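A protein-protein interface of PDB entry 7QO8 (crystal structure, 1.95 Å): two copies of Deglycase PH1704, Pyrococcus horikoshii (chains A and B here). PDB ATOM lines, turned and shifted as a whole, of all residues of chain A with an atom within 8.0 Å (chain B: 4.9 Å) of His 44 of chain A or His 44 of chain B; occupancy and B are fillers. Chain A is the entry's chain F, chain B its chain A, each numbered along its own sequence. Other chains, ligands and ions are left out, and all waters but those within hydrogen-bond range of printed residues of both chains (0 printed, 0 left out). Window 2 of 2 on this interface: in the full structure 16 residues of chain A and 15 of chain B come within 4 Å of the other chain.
The side-chain amino group of Lys 43 of chain A lies within salt-bridge range of the side-chain carboxylate of Glu 12 of chain A. NZ of Lys 43 of chain B is in salt-bridge range of OE1 of Glu 12 of chain B (3.0 Å). The side-chain carboxylate (OD2) of Asp 13 of chain B is in hydrogen-bond range of the backbone NH (N) of Tyr 46 of chain B, at 3.0 Å. The backbone NH of Gly 45 of chain B is in hydrogen-bond range of the side-chain carboxylate of Asp 13 of chain B. OD1 of Asp 13 of chain A is in hydrogen-bond range of N of Tyr 46 of chain A (2.9 Å). OD1 of Asp 13 of chain B lies within hydrogen-bond range of N of Lys 43 of chain B, at 3.1 Å.
Of the printed residues of chain B, His 44 of chain A touches His 44 (3.0 Å) and Tyr 46 (3.3 Å). His 44 of chain B touches two residues of chain A. Printed residues of chain B within 4 Å of Asp 13 of chain A: Tyr 46. Printed residues of chain B within 4 Å of Glu 12 of chain A: Tyr 46 (2.5 Å). The nearest residue of chain B that does not touch His 44 of chain A is Gly 45 of chain B (4.1 Å). The nearest residue of chain A that does not touch His 44 of chain B is Gly 45 of chain A (4.2 Å). The nearest printed residue of chain A that does not touch Asp 13 of chain B is His 44 of chain A (5.6 Å).
Of the 14 printed residues of chain A, 5 touch a printed residue of chain B.
A ring nitrogen (ND1) of His 44 of chain A lies within hydrogen-bond range of the backbone carbonyl oxygen (O) of His 44 of chain B (3.0 Å). The side-chain hydroxyl (OH) of Tyr 46 of chain B lies within hydrogen-bond range of the side-chain carboxylate (OE2) of Glu 12 of chain A. OE2 of Glu 12 of chain B lies within hydrogen-bond range of OH of Tyr 46 of chain A (2.5 Å). The side-chain hydroxyl (OH) of Tyr 46 of chain B sits at hydrogen-bond distance from the backbone NH (N) of Val 14 of chain A (3.1 Å). The side-chain hydroxyl of Tyr 46 of chain A lies close to the backbone NH of Asp 13 of chain B (3.3 Å). The side-chain hydroxyl (OH) of Tyr 46 of chain B is in hydrogen-bond range of the backbone NH (N) of Asp 13 of chain A (3.3 Å).
CD2 of His 44 of chain A touches OH of Tyr 46 of chain B, 3.3 Å away. OH of Tyr 46 of chain A touches CD2 of His 44 of chain B, 3.4 Å away.
Glu 12 of chain A touches Tyr 46 of chain B, and with the chains exchanged Tyr 46 of chain A touches Glu 12 of chain B. Asp 13 of chain A touches Tyr 46 of chain B, and with the chains exchanged Tyr 46 of chain A touches Asp 13 of chain B. His 44 of chain B touches its own counterpart, His 44 of chain A. His 44 of chain A touches Tyr 46 of chain B, and with the chains exchanged Tyr 46 of chain A touches His 44 of chain B. Positions printed for both chains: 12, 13, 42, 43, 44, 45 and 46.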
ATOM      1  N   GLU A  10       3.872  35.191  -2.393  1.00  0.00           N
ATOM      2  CA  GLU A  10       3.066  34.240  -3.200  1.00  0.00           C
ATOM      3  C   GLU A  10       3.893  33.649  -4.345  1.00  0.00           C
ATOM      4  O   GLU A  10       3.296  33.213  -5.318  1.00  0.00           O
ATOM      5  CB  GLU A  10       1.696  34.820  -3.559  1.00  0.00           C
ATOM      6  CG  GLU A  10       0.800  35.032  -2.353  1.00  0.00           C
ATOM      7  CD  GLU A  10       0.569  33.798  -1.497  1.00  0.00           C
ATOM      8  OE1 GLU A  10      -0.208  32.928  -1.923  1.00  0.00           O
ATOM      9  OE2 GLU A  10       1.166  33.712  -0.409  1.00  0.00           O
ATOM     10  N   PHE A  11       5.221  33.688  -4.229  1.00  0.00           N
ATOM     11  CA  PHE A  11       6.011  32.922  -5.185  1.00  0.00           C
ATOM     12  C   PHE A  11       5.711  31.443  -5.014  1.00  0.00           C
ATOM     13  O   PHE A  11       5.231  31.004  -3.966  1.00  0.00           O
ATOM     14  CB  PHE A  11       7.511  33.185  -5.004  1.00  0.00           C
ATOM     15  CG  PHE A  11       8.050  32.819  -3.619  1.00  0.00           C
ATOM     16  CD1 PHE A  11       8.575  31.565  -3.376  1.00  0.00           C
ATOM     17  CD2 PHE A  11       8.032  33.745  -2.591  1.00  0.00           C
ATOM     18  CE1 PHE A  11       9.066  31.224  -2.097  1.00  0.00           C
ATOM     19  CE2 PHE A  11       8.529  33.429  -1.320  1.00  0.00           C
ATOM     20  CZ  PHE A  11       9.040  32.167  -1.079  1.00  0.00           C
ATOM     21  N   GLU A  12       5.925  30.684  -6.083  1.00  0.00           N
ATOM     22  CA  GLU A  12       5.828  29.230  -6.005  1.00  0.00           C
ATOM     23  C   GLU A  12       7.065  28.691  -5.301  1.00  0.00           C
ATOM     24  O   GLU A  12       8.183  28.848  -5.805  1.00  0.00           O
ATOM     25  CB  GLU A  12       5.701  28.633  -7.398  1.00  0.00           C
ATOM     26  CG  GLU A  12       5.786  27.129  -7.374  1.00  0.00           C
ATOM     27  CD  GLU A  12       4.618  26.517  -6.675  1.00  0.00           C
ATOM     28  OE1 GLU A  12       3.497  27.058  -6.817  1.00  0.00           O
ATOM     29  OE2 GLU A  12       4.803  25.495  -5.992  1.00  0.00           O
ATOM     30  N   ASP A  13       6.871  28.066  -4.129  1.00  0.00           N
ATOM     31  CA  ASP A  13       7.983  27.887  -3.191  1.00  0.00           C
ATOM     32  C   ASP A  13       9.144  27.149  -3.829  1.00  0.00           C
ATOM     33  O   ASP A  13      10.300  27.609  -3.768  1.00  0.00           O
ATOM     34  CB  ASP A  13       7.515  27.149  -1.925  1.00  0.00           C
ATOM     35  CG  ASP A  13       6.334  27.840  -1.253  1.00  0.00           C
ATOM     36  OD1 ASP A  13       6.461  28.190  -0.069  1.00  0.00           O
ATOM     37  OD2 ASP A  13       5.303  28.057  -1.919  1.00  0.00           O
ATOM     38  N   VAL A  14       8.872  25.980  -4.417  1.00  0.00           N
ATOM     39  CA  VAL A  14       9.987  25.189  -4.916  1.00  0.00           C
ATOM     40  C   VAL A  14      10.583  25.819  -6.157  1.00  0.00           C
ATOM     41  O   VAL A  14      11.757  25.604  -6.459  1.00  0.00           O
ATOM     42  CB  VAL A  14       9.575  23.724  -5.152  1.00  0.00           C
ATOM     43  CG1 VAL A  14       9.144  23.101  -3.844  1.00  0.00           C
ATOM     44  CG2 VAL A  14       8.471  23.595  -6.220  1.00  0.00           C
ATOM     45  N   ILE A  17      13.080  28.044  -4.358  1.00  0.00           N
ATOM     46  CA  ILE A  17      14.052  27.402  -3.479  1.00  0.00           C
ATOM     47  C   ILE A  17      14.970  26.473  -4.268  1.00  0.00           C
ATOM     48  O   ILE A  17      16.175  26.421  -4.017  1.00  0.00           O
ATOM     49  CB  ILE A  17      13.315  26.688  -2.328  1.00  0.00           C
ATOM     50  CG1 ILE A  17      12.733  27.745  -1.386  1.00  0.00           C
ATOM     51  CG2 ILE A  17      14.268  25.747  -1.556  1.00  0.00           C
ATOM     52  CD1 ILE A  17      11.578  27.242  -0.470  1.00  0.00           C
ATOM     53  N   THR A  41       6.952  35.378   1.590  1.00  0.00           N
ATOM     54  CA  THR A  41       6.434  34.042   1.873  1.00  0.00           C
ATOM     55  C   THR A  41       5.811  33.434   0.624  1.00  0.00           C
ATOM     56  O   THR A  41       5.000  34.080  -0.059  1.00  0.00           O
ATOM     57  CB  THR A  41       5.403  34.094   3.011  1.00  0.00           C
ATOM     58  OG1 THR A  41       5.958  34.830   4.103  1.00  0.00           O
ATOM     59  CG2 THR A  41       5.053  32.695   3.507  1.00  0.00           C
ATOM     60  N   GLY A  42       6.160  32.176   0.347  1.00  0.00           N
ATOM     61  CA  GLY A  42       5.609  31.503  -0.809  1.00  0.00           C
ATOM     62  C   GLY A  42       4.174  31.040  -0.605  1.00  0.00           C
ATOM     63  O   GLY A  42       3.619  31.101   0.491  1.00  0.00           O
ATOM     64  N   LYS A  43       3.576  30.591  -1.720  1.00  0.00           N
ATOM     65  CA  LYS A  43       2.218  30.048  -1.713  1.00  0.00           C
ATOM     66  C   LYS A  43       2.041  28.965  -0.655  1.00  0.00           C
ATOM     67  O   LYS A  43       0.978  28.858  -0.033  1.00  0.00           O
ATOM     68  CB  LYS A  43       1.883  29.480  -3.095  1.00  0.00           C
ATOM     69  CG  LYS A  43       1.600  30.536  -4.134  1.00  0.00           C
ATOM     70  CD  LYS A  43       1.613  29.951  -5.551  1.00  0.00           C
ATOM     71  CE  LYS A  43       0.694  28.746  -5.679  1.00  0.00           C
ATOM     72  NZ  LYS A  43       0.741  28.153  -7.056  1.00  0.00           N
ATOM     73  N   HIS A  44       3.068  28.141  -0.457  1.00  0.00           N
ATOM     74  CA  HIS A  44       3.019  27.003   0.460  1.00  0.00           C
ATOM     75  C   HIS A  44       3.612  27.299   1.828  1.00  0.00           C
ATOM     76  O   HIS A  44       3.780  26.367   2.627  1.00  0.00           O
ATOM     77  CB  HIS A  44       3.742  25.802  -0.137  1.00  0.00           C
ATOM     78  CG  HIS A  44       3.040  25.216  -1.316  1.00  0.00           C
ATOM     79  ND1 HIS A  44       2.152  24.169  -1.205  1.00  0.00           N
ATOM     80  CD2 HIS A  44       3.089  25.538  -2.631  1.00  0.00           C
ATOM     81  CE1 HIS A  44       1.690  23.866  -2.406  1.00  0.00           C
ATOM     82  NE2 HIS A  44       2.248  24.676  -3.287  1.00  0.00           N
ATOM     83  N   GLY A  45       3.956  28.551   2.116  1.00  0.00           N
ATOM     84  CA  GLY A  45       4.330  28.943   3.463  1.00  0.00           C
ATOM     85  C   GLY A  45       5.815  29.015   3.771  1.00  0.00           C
ATOM     86  O   GLY A  45       6.172  29.379   4.892  1.00  0.00           O
ATOM     87  N   TYR A  46       6.692  28.702   2.823  1.00  0.00           N
ATOM     88  CA  TYR A  46       8.118  28.905   3.048  1.00  0.00           C
ATOM     89  C   TYR A  46       8.459  30.394   3.083  1.00  0.00           C
ATOM     90  O   TYR A  46       7.946  31.188   2.289  1.00  0.00           O
ATOM     91  CB  TYR A  46       8.934  28.215   1.960  1.00  0.00           C
ATOM     92  CG  TYR A  46       9.065  26.713   2.141  1.00  0.00           C
ATOM     93  CD1 TYR A  46      10.043  26.167   2.983  1.00  0.00           C
ATOM     94  CD2 TYR A  46       8.227  25.841   1.463  1.00  0.00           C
ATOM     95  CE1 TYR A  46      10.175  24.787   3.144  1.00  0.00           C
ATOM     96  CE2 TYR A  46       8.354  24.433   1.627  1.00  0.00           C
ATOM     97  CZ  TYR A  46       9.331  23.929   2.474  1.00  0.00           C
ATOM     98  OH  TYR A  46       9.463  22.564   2.620  1.00  0.00           O
ATOM     99  N   SER A  47       9.331  30.770   4.016  1.00  0.00           N
ATOM    100  CA  SER A  47       9.789  32.145   4.155  1.00  0.00           C
ATOM    101  C   SER A  47      11.200  32.284   3.603  1.00  0.00           C
ATOM    102  O   SER A  47      12.065  31.433   3.832  1.00  0.00           O
ATOM    103  CB  SER A  47       9.766  32.586   5.617  1.00  0.00           C
ATOM    104  OG  SER A  47       8.477  33.069   5.934  1.00  0.00           O
ATOM    105  N   PRO A 151       6.526  22.715 -11.624  1.00  0.00           N
ATOM    106  CA  PRO A 151       7.547  22.134 -10.722  1.00  0.00           C
ATOM    107  C   PRO A 151       8.073  20.768 -11.143  1.00  0.00           C
ATOM    108  O   PRO A 151       9.244  20.484 -10.877  1.00  0.00           O
ATOM    109  CB  PRO A 151       6.819  22.074  -9.371  1.00  0.00           C
ATOM    110  CG  PRO A 151       5.888  23.279  -9.431  1.00  0.00           C
ATOM    111  CD  PRO A 151       5.380  23.277 -10.873  1.00  0.00           C
ATOM    112  N   GLU B  12       9.199  16.817   5.061  1.00  0.00           N
ATOM    113  CA  GLU B  12       9.565  18.210   4.837  1.00  0.00           C
ATOM    114  C   GLU B  12       9.703  18.446   3.340  1.00  0.00           C
ATOM    115  O   GLU B  12      10.561  17.838   2.693  1.00  0.00           O
ATOM    116  CB  GLU B  12      10.863  18.542   5.569  1.00  0.00           C
ATOM    117  CG  GLU B  12      11.437  19.875   5.136  1.00  0.00           C
ATOM    118  CD  GLU B  12      10.584  21.040   5.555  1.00  0.00           C
ATOM    119  OE1 GLU B  12      10.015  20.991   6.669  1.00  0.00           O
ATOM    120  OE2 GLU B  12      10.505  22.014   4.778  1.00  0.00           O
ATOM    121  N   ASP B  13       8.855  19.316   2.788  1.00  0.00           N
ATOM    122  CA  ASP B  13       8.607  19.315   1.341  1.00  0.00           C
ATOM    123  C   ASP B  13       9.883  19.483   0.529  1.00  0.00           C
ATOM    124  O   ASP B  13      10.152  18.684  -0.373  1.00  0.00           O
ATOM    125  CB  ASP B  13       7.592  20.396   0.985  1.00  0.00           C
ATOM    126  CG  ASP B  13       6.299  20.225   1.744  1.00  0.00           C
ATOM    127  OD1 ASP B  13       6.369  20.170   3.001  1.00  0.00           O
ATOM    128  OD2 ASP B  13       5.225  20.128   1.101  1.00  0.00           O
ATOM    129  N   GLY B  42       3.401  16.574   1.837  1.00  0.00           N
ATOM    130  CA  GLY B  42       4.353  17.133   2.772  1.00  0.00           C
ATOM    131  C   GLY B  42       3.715  18.076   3.781  1.00  0.00           C
ATOM    132  O   GLY B  42       2.537  18.433   3.685  1.00  0.00           O
ATOM    133  N   LYS B  43       4.534  18.470   4.766  1.00  0.00           N
ATOM    134  CA  LYS B  43       4.124  19.434   5.785  1.00  0.00           C
ATOM    135  C   LYS B  43       3.511  20.688   5.172  1.00  0.00           C
ATOM    136  O   LYS B  43       2.563  21.261   5.725  1.00  0.00           O
ATOM    137  CB  LYS B  43       5.334  19.859   6.631  1.00  0.00           C
ATOM    138  CG  LYS B  43       5.872  18.853   7.628  1.00  0.00           C
ATOM    139  CD  LYS B  43       7.257  19.304   8.109  1.00  0.00           C
ATOM    140  CE  LYS B  43       7.290  20.806   8.395  1.00  0.00           C
ATOM    141  NZ  LYS B  43       8.473  21.216   9.210  1.00  0.00           N
ATOM    142  N   HIS B  44       4.070  21.153   4.054  1.00  0.00           N
ATOM    143  CA  HIS B  44       3.640  22.392   3.418  1.00  0.00           C
ATOM    144  C   HIS B  44       2.659  22.170   2.269  1.00  0.00           C
ATOM    145  O   HIS B  44       2.343  23.123   1.553  1.00  0.00           O
ATOM    146  CB  HIS B  44       4.852  23.164   2.907  1.00  0.00           C
ATOM    147  CG  HIS B  44       5.766  23.646   3.988  1.00  0.00           C
ATOM    148  ND1 HIS B  44       5.702  24.922   4.507  1.00  0.00           N
ATOM    149  CD2 HIS B  44       6.776  23.023   4.643  1.00  0.00           C
ATOM    150  CE1 HIS B  44       6.635  25.063   5.435  1.00  0.00           C
ATOM    151  NE2 HIS B  44       7.298  23.927   5.534  1.00  0.00           N
ATOM    152  N   GLY B  45       2.192  20.943   2.061  1.00  0.00           N
ATOM    153  CA  GLY B  45       1.111  20.688   1.136  1.00  0.00           C
ATOM    154  C   GLY B  45       1.488  20.226  -0.257  1.00  0.00           C
ATOM    155  O   GLY B  45       0.590  20.002  -1.063  1.00  0.00           O
ATOM    156  N   TYR B  46       2.767  20.087  -0.580  1.00  0.00           N
ATOM    157  CA  TYR B  46       3.125  19.488  -1.861  1.00  0.00           C
ATOM    158  C   TYR B  46       2.801  18.000  -1.837  1.00  0.00           C
ATOM    159  O   TYR B  46       3.029  17.309  -0.838  1.00  0.00           O
ATOM    160  CB  TYR B  46       4.610  19.690  -2.169  1.00  0.00           C
ATOM    161  CG  TYR B  46       4.988  21.079  -2.634  1.00  0.00           C
ATOM    162  CD1 TYR B  46       4.817  21.466  -3.968  1.00  0.00           C
ATOM    163  CD2 TYR B  46       5.521  22.003  -1.744  1.00  0.00           C
ATOM    164  CE1 TYR B  46       5.164  22.744  -4.398  1.00  0.00           C
ATOM    165  CE2 TYR B  46       5.870  23.276  -2.156  1.00  0.00           C
ATOM    166  CZ  TYR B  46       5.692  23.646  -3.487  1.00  0.00           C
ATOM    167  OH  TYR B  46       6.050  24.920  -3.877  1.00  0.00           O
